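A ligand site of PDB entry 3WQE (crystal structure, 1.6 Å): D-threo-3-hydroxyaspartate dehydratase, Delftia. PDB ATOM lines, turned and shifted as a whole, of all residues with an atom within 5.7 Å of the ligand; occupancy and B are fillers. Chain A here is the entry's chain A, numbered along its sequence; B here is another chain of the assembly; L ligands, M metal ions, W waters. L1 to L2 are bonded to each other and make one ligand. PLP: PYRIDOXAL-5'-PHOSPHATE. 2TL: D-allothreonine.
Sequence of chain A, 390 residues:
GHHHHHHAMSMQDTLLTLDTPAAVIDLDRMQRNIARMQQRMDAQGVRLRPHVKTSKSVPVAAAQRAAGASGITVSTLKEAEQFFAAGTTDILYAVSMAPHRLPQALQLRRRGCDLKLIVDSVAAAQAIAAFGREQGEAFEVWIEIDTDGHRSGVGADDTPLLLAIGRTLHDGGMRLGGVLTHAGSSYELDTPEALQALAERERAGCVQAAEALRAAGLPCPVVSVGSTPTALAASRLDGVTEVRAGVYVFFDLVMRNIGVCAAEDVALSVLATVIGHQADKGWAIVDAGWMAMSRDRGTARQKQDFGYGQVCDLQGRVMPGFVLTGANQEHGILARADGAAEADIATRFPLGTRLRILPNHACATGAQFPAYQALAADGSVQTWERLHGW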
ATOM      1  N   HIS A  51     -37.146 -28.889  11.173  1.00  0.00           N
ATOM      2  CA  HIS A  51     -36.691 -29.155  12.548  1.00  0.00           C
ATOM      3  C   HIS A  51     -37.543 -28.325  13.510  1.00  0.00           C
ATOM      4  O   HIS A  51     -37.420 -27.081  13.572  1.00  0.00           O
ATOM      5  CB  HIS A  51     -35.218 -28.805  12.676  1.00  0.00           C
ATOM      6  CG  HIS A  51     -34.606 -29.597  13.807  1.00  0.00           C
ATOM      7  ND1 HIS A  51     -35.325 -29.846  14.973  1.00  0.00           N
ATOM      8  CD2 HIS A  51     -33.455 -30.361  13.892  1.00  0.00           C
ATOM      9  CE1 HIS A  51     -34.608 -30.678  15.759  1.00  0.00           C
ATOM     10  NE2 HIS A  51     -33.471 -31.005  15.121  1.00  0.00           N
ATOM     11  N   LYS A  53     -37.435 -28.147  16.584  1.00  0.00           N
ATOM     12  CA  LYS A  53     -36.812 -27.699  17.893  1.00  0.00           C
ATOM     13  C   LYS A  53     -36.831 -26.155  17.992  1.00  0.00           C
ATOM     14  O   LYS A  53     -36.693 -25.673  19.107  1.00  0.00           O
ATOM     15  CB  LYS A  53     -35.397 -28.213  18.074  1.00  0.00           C
ATOM     16  CG  LYS A  53     -34.351 -27.519  17.212  1.00  0.00           C
ATOM     17  CD  LYS A  53     -32.966 -28.064  17.554  1.00  0.00           C
ATOM     18  CE  LYS A  53     -31.926 -27.508  16.584  1.00  0.00           C
ATOM     19  NZ  LYS A  53     -32.011 -26.054  16.520  1.00  0.00           N
ATOM     20  N   THR A  54     -36.984 -25.429  16.868  1.00  0.00           N
ATOM     21  CA  THR A  54     -37.025 -23.955  16.929  1.00  0.00           C
ATOM     22  C   THR A  54     -38.283 -23.503  17.661  1.00  0.00           C
ATOM     23  O   THR A  54     -38.180 -22.550  18.449  1.00  0.00           O
ATOM     24  CB  THR A  54     -36.999 -23.415  15.490  1.00  0.00           C
ATOM     25  OG1 THR A  54     -35.676 -23.675  14.975  1.00  0.00           O
ATOM     26  CG2 THR A  54     -37.176 -21.882  15.520  1.00  0.00           C
ATOM     27  N   THR A  73     -38.265 -33.231  12.175  1.00  0.00           N
ATOM     28  CA  THR A  73     -37.074 -33.597  12.919  1.00  0.00           C
ATOM     29  C   THR A  73     -37.302 -33.042  14.307  1.00  0.00           C
ATOM     30  O   THR A  73     -37.814 -31.935  14.475  1.00  0.00           O
ATOM     31  CB  THR A  73     -35.839 -32.861  12.356  1.00  0.00           C
ATOM     32  OG1 THR A  73     -35.786 -33.117  10.926  1.00  0.00           O
ATOM     33  CG2 THR A  73     -34.529 -33.551  12.909  1.00  0.00           C
ATOM     34  N   ALA A  94     -33.033 -36.512  15.774  1.00  0.00           N
ATOM     35  CA  ALA A  94     -31.721 -36.318  15.190  1.00  0.00           C
ATOM     36  C   ALA A  94     -30.678 -35.913  16.221  1.00  0.00           C
ATOM     37  O   ALA A  94     -29.971 -34.898  16.042  1.00  0.00           O
ATOM     38  CB  ALA A  94     -31.771 -35.278  14.041  1.00  0.00           C
ATOM     39  N   GLU A 144     -25.159 -40.947  11.191  1.00  0.00           N
ATOM     40  CA  GLU A 144     -24.844 -39.499  11.104  1.00  0.00           C
ATOM     41  C   GLU A 144     -23.387 -39.361  10.550  1.00  0.00           C
ATOM     42  O   GLU A 144     -22.471 -40.048  11.004  1.00  0.00           O
ATOM     43  CB  GLU A 144     -24.912 -38.851  12.501  1.00  0.00           C
ATOM     44  CG  GLU A 144     -24.746 -37.363  12.391  1.00  0.00           C
ATOM     45  CD  GLU A 144     -25.096 -36.616  13.679  1.00  0.00           C
ATOM     46  OE1 GLU A 144     -25.406 -35.428  13.590  1.00  0.00           O
ATOM     47  OE2 GLU A 144     -25.096 -37.206  14.791  1.00  0.00           O
ATOM     48  N   HIS A 150     -18.111 -29.969  12.421  1.00  0.00           N
ATOM     49  CA  HIS A 150     -18.828 -29.147  13.398  1.00  0.00           C
ATOM     50  C   HIS A 150     -18.999 -29.851  14.737  1.00  0.00           C
ATOM     51  O   HIS A 150     -18.921 -29.188  15.773  1.00  0.00           O
ATOM     52  CB  HIS A 150     -20.236 -28.906  12.760  1.00  0.00           C
ATOM     53  CG  HIS A 150     -21.215 -28.279  13.647  1.00  0.00           C
ATOM     54  ND1 HIS A 150     -21.075 -26.991  14.087  1.00  0.00           N
ATOM     55  CD2 HIS A 150     -22.432 -28.753  14.137  1.00  0.00           C
ATOM     56  CE1 HIS A 150     -22.179 -26.673  14.855  1.00  0.00           C
ATOM     57  NE2 HIS A 150     -22.988 -27.735  14.874  1.00  0.00           N
ATOM     58  N   ARG A 151     -19.316 -31.129  14.738  1.00  0.00           N
ATOM     59  CA  ARG A 151     -20.015 -31.854  15.897  1.00  0.00           C
ATOM     60  C   ARG A 151     -19.984 -33.418  15.745  1.00  0.00           C
ATOM     61  O   ARG A 151     -18.929 -33.966  15.664  1.00  0.00           O
ATOM     62  CB  ARG A 151     -21.425 -31.367  16.118  1.00  0.00           C
ATOM     63  CG  ARG A 151     -22.147 -31.777  17.428  1.00  0.00           C
ATOM     64  CD  ARG A 151     -23.423 -30.964  17.512  1.00  0.00           C
ATOM     65  NE  ARG A 151     -24.463 -31.503  16.589  1.00  0.00           N
ATOM     66  CZ  ARG A 151     -25.549 -30.823  16.211  1.00  0.00           C
ATOM     67  NH1 ARG A 151     -25.673 -29.472  16.645  1.00  0.00           N
ATOM     68  NH2 ARG A 151     -26.546 -31.430  15.407  1.00  0.00           N
ATOM     69  N   LEU A 180     -27.434 -39.071   7.375  1.00  0.00           N
ATOM     70  CA  LEU A 180     -27.797 -37.643   7.486  1.00  0.00           C
ATOM     71  C   LEU A 180     -26.560 -36.868   7.932  1.00  0.00           C
ATOM     72  O   LEU A 180     -25.631 -37.426   8.522  1.00  0.00           O
ATOM     73  CB  LEU A 180     -28.956 -37.372   8.492  1.00  0.00           C
ATOM     74  CG  LEU A 180     -28.584 -37.409   9.984  1.00  0.00           C
ATOM     75  CD1 LEU A 180     -29.742 -36.777  10.770  1.00  0.00           C
ATOM     76  CD2 LEU A 180     -28.330 -38.845  10.442  1.00  0.00           C
ATOM     77  N   THR A 181     -26.592 -35.598   7.589  1.00  0.00           N
ATOM     78  CA  THR A 181     -25.494 -34.714   8.043  1.00  0.00           C
ATOM     79  C   THR A 181     -26.095 -33.368   8.300  1.00  0.00           C
ATOM     80  O   THR A 181     -27.139 -32.986   7.718  1.00  0.00           O
ATOM     81  CB  THR A 181     -24.333 -34.646   6.982  1.00  0.00           C
ATOM     82  OG1 THR A 181     -23.211 -33.981   7.609  1.00  0.00           O
ATOM     83  CG2 THR A 181     -24.840 -33.897   5.711  1.00  0.00           C
ATOM     84  N   HIS A 182     -25.398 -32.564   9.129  1.00  0.00           N
ATOM     85  CA  HIS A 182     -25.770 -31.193   9.398  1.00  0.00           C
ATOM     86  C   HIS A 182     -24.526 -30.341   9.358  1.00  0.00           C
ATOM     87  O   HIS A 182     -23.621 -30.546  10.197  1.00  0.00           O
ATOM     88  CB  HIS A 182     -26.396 -31.115  10.806  1.00  0.00           C
ATOM     89  CG  HIS A 182     -26.558 -29.724  11.306  1.00  0.00           C
ATOM     90  ND1 HIS A 182     -27.439 -28.817  10.782  1.00  0.00           N
ATOM     91  CD2 HIS A 182     -25.945 -29.089  12.450  1.00  0.00           C
ATOM     92  CE1 HIS A 182     -27.391 -27.646  11.546  1.00  0.00           C
ATOM     93  NE2 HIS A 182     -26.441 -27.835  12.520  1.00  0.00           N
ATOM     94  N   GLY A 184     -23.212 -27.627  10.426  1.00  0.00           N
ATOM     95  CA  GLY A 184     -23.467 -26.503  11.365  1.00  0.00           C
ATOM     96  C   GLY A 184     -22.348 -25.471  11.308  1.00  0.00           C
ATOM     97  O   GLY A 184     -22.536 -24.336  11.917  1.00  0.00           O
ATOM     98  N   TYR A 187     -22.885 -21.567  10.330  1.00  0.00           N
ATOM     99  CA  TYR A 187     -23.206 -20.385  11.185  1.00  0.00           C
ATOM    100  C   TYR A 187     -22.001 -19.479  11.314  1.00  0.00           C
ATOM    101  O   TYR A 187     -22.196 -18.329  11.767  1.00  0.00           O
ATOM    102  CB  TYR A 187     -23.675 -20.968  12.512  1.00  0.00           C
ATOM    103  CG  TYR A 187     -25.149 -21.362  12.490  1.00  0.00           C
ATOM    104  CD1 TYR A 187     -25.621 -22.388  11.725  1.00  0.00           C
ATOM    105  CD2 TYR A 187     -26.014 -20.701  13.358  1.00  0.00           C
ATOM    106  CE1 TYR A 187     -26.968 -22.778  11.767  1.00  0.00           C
ATOM    107  CE2 TYR A 187     -27.389 -21.014  13.411  1.00  0.00           C
ATOM    108  CZ  TYR A 187     -27.839 -22.085  12.604  1.00  0.00           C
ATOM    109  OH  TYR A 187     -29.188 -22.354  12.653  1.00  0.00           O
ATOM    110  N   GLY A 226     -28.689 -30.701   5.886  1.00  0.00           N
ATOM    111  CA  GLY A 226     -29.299 -29.367   6.055  1.00  0.00           C
ATOM    112  C   GLY A 226     -28.865 -28.573   7.277  1.00  0.00           C
ATOM    113  O   GLY A 226     -28.709 -29.126   8.369  1.00  0.00           O
ATOM    114  N   SER A 227     -28.892 -27.289   7.013  1.00  0.00           N
ATOM    115  CA  SER A 227     -28.999 -26.238   8.029  1.00  0.00           C
ATOM    116  C   SER A 227     -29.733 -25.157   7.337  1.00  0.00           C
ATOM    117  O   SER A 227     -29.823 -25.172   6.088  1.00  0.00           O
ATOM    118  CB  SER A 227     -27.568 -25.750   8.450  1.00  0.00           C
ATOM    119  OG  SER A 227     -26.864 -25.086   7.389  1.00  0.00           O
ATOM    120  N   THR A 228     -30.257 -24.176   8.053  1.00  0.00           N
ATOM    121  CA  THR A 228     -31.006 -23.129   7.322  1.00  0.00           C
ATOM    122  C   THR A 228     -30.100 -22.420   6.286  1.00  0.00           C
ATOM    123  O   THR A 228     -30.533 -22.218   5.112  1.00  0.00           O
ATOM    124  CB  THR A 228     -31.742 -22.135   8.251  1.00  0.00           C
ATOM    125  OG1 THR A 228     -32.948 -22.792   8.701  1.00  0.00           O
ATOM    126  CG2 THR A 228     -32.107 -20.839   7.550  1.00  0.00           C
ATOM    127  N   PRO A 229     -28.844 -22.009   6.643  1.00  0.00           N
ATOM    128  CA  PRO A 229     -28.045 -21.280   5.664  1.00  0.00           C
ATOM    129  C   PRO A 229     -27.653 -22.140   4.437  1.00  0.00           C
ATOM    130  O   PRO A 229     -27.706 -21.653   3.285  1.00  0.00           O
ATOM    131  CB  PRO A 229     -26.751 -20.903   6.412  1.00  0.00           C
ATOM    132  CG  PRO A 229     -27.312 -20.780   7.871  1.00  0.00           C
ATOM    133  CD  PRO A 229     -28.255 -21.981   8.012  1.00  0.00           C
ATOM    134  N   ARG A 244     -33.252 -30.845   6.039  1.00  0.00           N
ATOM    135  CA  ARG A 244     -33.761 -30.458   7.363  1.00  0.00           C
ATOM    136  C   ARG A 244     -33.390 -29.043   7.651  1.00  0.00           C
ATOM    137  O   ARG A 244     -32.225 -28.665   7.437  1.00  0.00           O
ATOM    138  CB  ARG A 244     -33.138 -31.322   8.457  1.00  0.00           C
ATOM    139  CG  ARG A 244     -33.309 -32.824   8.130  1.00  0.00           C
ATOM    140  CD  ARG A 244     -32.740 -33.695   9.280  1.00  0.00           C
ATOM    141  NE  ARG A 244     -31.494 -33.125   9.767  1.00  0.00           N
ATOM    142  CZ  ARG A 244     -30.323 -33.204   9.047  1.00  0.00           C
ATOM    143  NH1 ARG A 244     -30.185 -33.981   7.937  1.00  0.00           N
ATOM    144  NH2 ARG A 244     -29.303 -32.442   9.461  1.00  0.00           N
ATOM    145  N   ALA A 245     -34.393 -28.223   7.989  1.00  0.00           N
ATOM    146  CA  ALA A 245     -34.068 -26.824   8.361  1.00  0.00           C
ATOM    147  C   ALA A 245     -35.135 -26.451   9.386  1.00  0.00           C
ATOM    148  O   ALA A 245     -36.321 -26.915   9.296  1.00  0.00           O
ATOM    149  CB  ALA A 245     -34.203 -25.866   7.154  1.00  0.00           C
ATOM    150  N   GLY A 246     -34.741 -25.551  10.316  1.00  0.00           N
ATOM    151  CA  GLY A 246     -35.716 -25.201  11.385  1.00  0.00           C
ATOM    152  C   GLY A 246     -35.756 -23.699  11.682  1.00  0.00           C
ATOM    153  O   GLY A 246     -36.888 -23.170  11.777  1.00  0.00           O
ATOM    154  N   VAL A 247     -34.571 -23.057  11.861  1.00  0.00           N
ATOM    155  CA  VAL A 247     -34.705 -21.662  12.345  1.00  0.00           C
ATOM    156  C   VAL A 247     -35.332 -20.735  11.314  1.00  0.00           C
ATOM    157  O   VAL A 247     -35.880 -19.704  11.695  1.00  0.00           O
ATOM    158  CB  VAL A 247     -33.332 -21.166  12.838  1.00  0.00           C
ATOM    159  CG1 VAL A 247     -32.327 -20.877  11.663  1.00  0.00           C
ATOM    160  CG2 VAL A 247     -33.511 -19.913  13.744  1.00  0.00           C
ATOM    161  N   TYR A 248     -35.330 -21.131  10.049  1.00  0.00           N
ATOM    162  CA  TYR A 248     -35.853 -20.255   9.007  1.00  0.00           C
ATOM    163  C   TYR A 248     -37.335 -19.882   9.254  1.00  0.00           C
ATOM    164  O   TYR A 248     -37.814 -18.945   8.676  1.00  0.00           O
ATOM    165  CB  TYR A 248     -35.779 -21.027   7.612  1.00  0.00           C
ATOM    166  CG  TYR A 248     -36.900 -22.080   7.522  1.00  0.00           C
ATOM    167  CD1 TYR A 248     -36.764 -23.333   8.103  1.00  0.00           C
ATOM    168  CD2 TYR A 248     -38.138 -21.733   6.926  1.00  0.00           C
ATOM    169  CE1 TYR A 248     -37.838 -24.271   8.048  1.00  0.00           C
ATOM    170  CE2 TYR A 248     -39.164 -22.671   6.826  1.00  0.00           C
ATOM    171  CZ  TYR A 248     -39.022 -23.900   7.434  1.00  0.00           C
ATOM    172  OH  TYR A 248     -40.047 -24.738   7.312  1.00  0.00           O
ATOM    173  N   MET A 255     -29.069 -15.125  11.632  1.00  0.00           N
ATOM    174  CA  MET A 255     -29.306 -15.417  10.193  1.00  0.00           C
ATOM    175  C   MET A 255     -29.204 -14.186   9.335  1.00  0.00           C
ATOM    176  O   MET A 255     -28.684 -14.281   8.189  1.00  0.00           O
ATOM    177  CB  MET A 255     -30.706 -16.050  10.042  1.00  0.00           C
ATOM    178  CG  MET A 255     -30.817 -17.454  10.684  1.00  0.00           C
ATOM    179  SD  MET A 255     -29.775 -18.663   9.723  1.00  0.00           S
ATOM    180  CE  MET A 255     -28.888 -19.273  11.153  1.00  0.00           C
ATOM    181  N   HIS A 361     -31.073 -15.264  18.458  1.00  0.00           N
ATOM    182  CA  HIS A 361     -31.206 -16.672  18.043  1.00  0.00           C
ATOM    183  C   HIS A 361     -32.598 -17.086  18.383  1.00  0.00           C
ATOM    184  O   HIS A 361     -32.998 -17.177  19.556  1.00  0.00           O
ATOM    185  CB  HIS A 361     -30.186 -17.448  18.907  1.00  0.00           C
ATOM    186  CG  HIS A 361     -30.134 -18.910  18.576  1.00  0.00           C
ATOM    187  ND1 HIS A 361     -29.262 -19.747  19.222  1.00  0.00           N
ATOM    188  CD2 HIS A 361     -30.765 -19.663  17.594  1.00  0.00           C
ATOM    189  CE1 HIS A 361     -29.372 -21.050  18.650  1.00  0.00           C
ATOM    190  NE2 HIS A 361     -30.244 -21.022  17.636  1.00  0.00           N
ATOM    191  N   CYS A 363     -34.259 -19.855  18.278  1.00  0.00           N
ATOM    192  CA  CYS A 363     -34.493 -21.120  19.031  1.00  0.00           C
ATOM    193  C   CYS A 363     -34.239 -20.879  20.525  1.00  0.00           C
ATOM    194  O   CYS A 363     -34.944 -21.459  21.353  1.00  0.00           O
ATOM    195  CB  CYS A 363     -33.401 -22.121  18.600  1.00  0.00           C
ATOM    196  SG  CYS A 363     -33.318 -22.281  16.738  1.00  0.00           S
ATOM    197  N   TRP B 290     -26.748 -26.133  25.344  1.00  0.00           N
ATOM    198  CA  TRP B 290     -27.122 -24.919  25.997  1.00  0.00           C
ATOM    199  C   TRP B 290     -28.594 -24.857  26.380  1.00  0.00           C
ATOM    200  O   TRP B 290     -29.015 -24.059  27.238  1.00  0.00           O
ATOM    201  CB  TRP B 290     -26.725 -23.632  25.153  1.00  0.00           C
ATOM    202  CG  TRP B 290     -27.391 -23.547  23.777  1.00  0.00           C
ATOM    203  CD1 TRP B 290     -26.786 -23.772  22.577  1.00  0.00           C
ATOM    204  CD2 TRP B 290     -28.819 -23.232  23.493  1.00  0.00           C
ATOM    205  NE1 TRP B 290     -27.677 -23.568  21.527  1.00  0.00           N
ATOM    206  CE2 TRP B 290     -28.922 -23.280  22.064  1.00  0.00           C
ATOM    207  CE3 TRP B 290     -29.964 -22.873  24.241  1.00  0.00           C
ATOM    208  CZ2 TRP B 290     -30.167 -23.063  21.449  1.00  0.00           C
ATOM    209  CZ3 TRP B 290     -31.218 -22.645  23.590  1.00  0.00           C
ATOM    210  CH2 TRP B 290     -31.266 -22.747  22.172  1.00  0.00           C
ATOM    211  N   ASN B 328     -24.158 -26.878  21.535  1.00  0.00           N
ATOM    212  CA  ASN B 328     -25.259 -26.572  20.650  1.00  0.00           C
ATOM    213  C   ASN B 328     -26.526 -26.900  21.407  1.00  0.00           C
ATOM    214  O   ASN B 328     -26.484 -27.087  22.615  1.00  0.00           O
ATOM    215  CB  ASN B 328     -25.162 -27.437  19.393  1.00  0.00           C
ATOM    216  CG  ASN B 328     -23.948 -26.999  18.491  1.00  0.00           C
ATOM    217  OD1 ASN B 328     -23.562 -27.749  17.734  1.00  0.00           O
ATOM    218  ND2 ASN B 328     -23.461 -25.769  18.634  1.00  0.00           N
ATOM    219  N   GLN B 329     -27.706 -26.806  20.757  1.00  0.00           N
ATOM    220  CA  GLN B 329     -28.931 -26.804  21.565  1.00  0.00           C
ATOM    221  C   GLN B 329     -29.069 -28.049  22.515  1.00  0.00           C
ATOM    222  O   GLN B 329     -29.370 -27.821  23.731  1.00  0.00           O
ATOM    223  CB  GLN B 329     -30.120 -26.737  20.562  1.00  0.00           C
ATOM    224  CG  GLN B 329     -31.423 -26.412  21.321  1.00  0.00           C
ATOM    225  CD  GLN B 329     -32.486 -25.941  20.393  1.00  0.00           C
ATOM    226  OE1 GLN B 329     -32.211 -25.155  19.464  1.00  0.00           O
ATOM    227  NE2 GLN B 329     -33.792 -26.297  20.662  1.00  0.00           N
ATOM    228  N   GLU B 330     -28.873 -29.220  21.946  1.00  0.00           N
ATOM    229  CA  GLU B 330     -29.021 -30.435  22.756  1.00  0.00           C
ATOM    230  C   GLU B 330     -27.738 -31.227  22.850  1.00  0.00           C
ATOM    231  O   GLU B 330     -27.806 -32.442  23.173  1.00  0.00           O
ATOM    232  CB  GLU B 330     -30.167 -31.342  22.210  1.00  0.00           C
ATOM    233  CG  GLU B 330     -31.561 -30.626  22.490  1.00  0.00           C
ATOM    234  CD  GLU B 330     -32.020 -30.503  23.976  1.00  0.00           C
ATOM    235  OE1 GLU B 330     -31.448 -31.229  24.857  1.00  0.00           O
ATOM    236  OE2 GLU B 330     -32.858 -29.627  24.255  1.00  0.00           O
ATOM    237  N   HIS B 331     -26.582 -30.655  22.430  1.00  0.00           N
ATOM    238  CA  HIS B 331     -25.347 -31.429  22.467  1.00  0.00           C
ATOM    239  C   HIS B 331     -24.351 -30.512  23.121  1.00  0.00           C
ATOM    240  O   HIS B 331     -24.230 -29.319  22.810  1.00  0.00           O
ATOM    241  CB  HIS B 331     -24.741 -31.614  21.084  1.00  0.00           C
ATOM    242  CG  HIS B 331     -25.538 -32.391  20.085  1.00  0.00           C
ATOM    243  ND1 HIS B 331     -26.639 -31.912  19.440  1.00  0.00           N
ATOM    244  CD2 HIS B 331     -25.287 -33.634  19.543  1.00  0.00           C
ATOM    245  CE1 HIS B 331     -27.098 -32.871  18.573  1.00  0.00           C
ATOM    246  NE2 HIS B 331     -26.256 -33.897  18.582  1.00  0.00           N
HETATM  247  N1  PLP L   1     -30.483 -30.872  11.692  1.00  0.00           N
HETATM  248  C2  PLP L   1     -29.789 -31.008  12.827  1.00  0.00           C
HETATM  249  C2A PLP L   1     -29.177 -32.349  13.175  1.00  0.00           C
HETATM  250  C3  PLP L   1     -29.479 -29.886  13.700  1.00  0.00           C
HETATM  251  O3  PLP L   1     -28.663 -30.062  14.757  1.00  0.00           O
HETATM  252  C4  PLP L   1     -30.013 -28.594  13.314  1.00  0.00           C
HETATM  253  C4A PLP L   1     -29.682 -27.337  14.094  1.00  0.00           C
HETATM  254  C5  PLP L   1     -30.864 -28.548  12.051  1.00  0.00           C
HETATM  255  C6  PLP L   1     -31.041 -29.729  11.265  1.00  0.00           C
HETATM  256  C5A PLP L   1     -31.583 -27.240  11.699  1.00  0.00           C
HETATM  257  O4P PLP L   1     -30.648 -26.195  11.382  1.00  0.00           O
HETATM  258  P   PLP L   1     -31.205 -24.738  11.348  1.00  0.00           P
HETATM  259  O1P PLP L   1     -32.278 -24.758  10.319  1.00  0.00           O
HETATM  260  O2P PLP L   1     -29.986 -23.986  10.870  1.00  0.00           O
HETATM  261  O3P PLP L   1     -31.672 -24.387  12.714  1.00  0.00           O
HETATM  262  N   2TL L   2     -28.610 -27.554  15.015  1.00  0.00           N
HETATM  263  CA  2TL L   2     -28.227 -26.246  15.765  1.00  0.00           C
HETATM  264  CB  2TL L   2     -26.844 -25.835  15.286  1.00  0.00           C
HETATM  265  OG1 2TL L   2     -26.658 -25.377  13.984  1.00  0.00           O
HETATM  266  CG2 2TL L   2     -25.829 -26.868  15.202  1.00  0.00           C
HETATM  267  C   2TL L   2     -28.105 -26.729  17.182  1.00  0.00           C
HETATM  268  O   2TL L   2     -27.927 -27.931  17.366  1.00  0.00           O
HETATM  269  OXT 2TL L   2     -28.085 -25.898  18.039  1.00  0.00           O
HETATM  270 MG    MG M   1     -30.689 -22.583  16.377  1.00  0.00          MG
HETATM  271  O   HOH W   1     -30.247 -23.955  17.932  1.00  0.00           O
HETATM  272  O   HOH W   2     -24.093 -24.261  14.355  1.00  0.00           O
HETATM  273  O   HOH W   3     -33.791 -25.629  14.111  1.00  0.00           O
HETATM  274  O   HOH W   4     -26.725 -23.673  18.874  1.00  0.00           O
HETATM  275  O   HOH W   5     -28.408 -22.809  15.994  1.00  0.00           O
HETATM  276  O   HOH W   6     -28.353 -29.697  19.192  1.00  0.00           O
HETATM  277  O   HOH W   7     -29.984 -30.490  17.176  1.00  0.00           O
HETATM  278  O   HOH W   8     -30.895 -24.145  14.978  1.00  0.00           O
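A ring nitrogen (ND1) of His 51 lies close to the backbone NH (N) of Lys 53, at 3.2 Å.
The backbone NH (N) of Val 247 sits at hydrogen-bond distance from the side-chain hydroxyl (OG1) of Thr 54 (3.4 Å).
OG1 of Thr 228 lies within hydrogen-bond range of N of Tyr 248 (3.2 Å).
NH2 of Arg 244 is in hydrogen-bond range of O of Thr 181, at 2.8 Å.
The guanidinium group of Arg 151 is in hydrogen-bond range of the side-chain amide oxygen of Asn 328 of chain B, 2.9 Å away.
OD1 of Asn 328 of chain B sits at hydrogen-bond distance from NE2 of His 150.
The backbone carbonyl oxygen (O) of Gly 246 sits close to the side-chain hydroxyl (OG1) of Thr 54 (3.5 Å).
The backbone carbonyl oxygen (O) of Asn 328 of chain B lies within hydrogen-bond range of the backbone NH (N) of Trp 290 of chain B (2.9 Å).
The backbone NH (N) of Thr 228 sits at hydrogen-bond distance from an oxygen (O2P) of PLP L1.
The side-chain hydroxyl of Thr 228 is in hydrogen-bond range of an oxygen (O1P) of PLP L1 (2.6 Å).
N of Val 247 is in hydrogen-bond range of O1P of PLP L1 (3.2 Å).
NH2 of Arg 244 lies within hydrogen-bond range of N1 of PLP L1 (3.0 Å).
OXT of 2TL L2 is in hydrogen-bond range of N of Gln 329 of chain B (2.9 Å).
An oxygen (O) of 2TL L2 is in salt-bridge range of the guanidinium group (NH1) of Arg 151, at 2.8 Å.
The backbone NH (N) of Gly 246 lies within hydrogen-bond range of an oxygen (O1P) of PLP L1, 2.6 Å away.
The side-chain hydroxyl (OH) of Tyr 187 is in hydrogen-bond range of an oxygen (O2P) of PLP L1, at 2.5 Å.
A ring nitrogen (NE2) of His 182 is in hydrogen-bond range of an oxygen (OG1) of 2TL L2 (2.9 Å).
Water W8 lies within hydrogen-bond range of an oxygen (O3P) of PLP L1 (2.4 Å), the side-chain amino group of Lys 53 (2.7 Å) and the side-chain hydroxyl of Tyr 187 (3.4 Å).
Water W6 lies within hydrogen-bond range of O of 2TL L2 (2.6 Å), ND1 of His 331 of chain B (2.8 Å), N of Glu 330 of chain B (2.8 Å) and N of Gln 329 of chain B (3.4 Å).
Water W4 lies within hydrogen-bond range of an oxygen (OXT) of 2TL L2 (2.7 Å) and the indole nitrogen of Trp 290 of chain B (2.8 Å).
Water W2 bridges OG1 of 2TL L2 (2.8 Å) and O of Gly 184 (2.9 Å).
Water W3 lies within hydrogen-bond range of an oxygen (O3P) of PLP L1 (2.8 Å), the side-chain hydroxyl of Thr 54 (2.8 Å) and the side-chain amino group of Lys 53 (3.0 Å).
Water W1 lies within hydrogen-bond range of OE1 of Gln 329 of chain B (2.8 Å), OXT of 2TL L2 (2.9 Å) and NZ of Lys 53 (3.1 Å).
His 51 touches the ligand.
Lys 53 touches the ligand.
O of Ala 94 touches C2A of PLP L1, at 3.9 Å.
His 150 touches the ligand.
O of Gly 226 touches C6 of PLP L1, at 3.8 Å.
Ser 227 touches the ligand.
CD of Pro 229 touches O2P of PLP L1, 3.9 Å away.
CA of Ala 245 touches O1P of PLP L1 (3.4 Å).
Asn 328 of chain B touches the ligand.
Of the 30 residues printed, 17 come within 4 Å of the ligand.
The nearest printed residue that does not touch the ligand is Trp 290 of chain B (4.2 Å).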
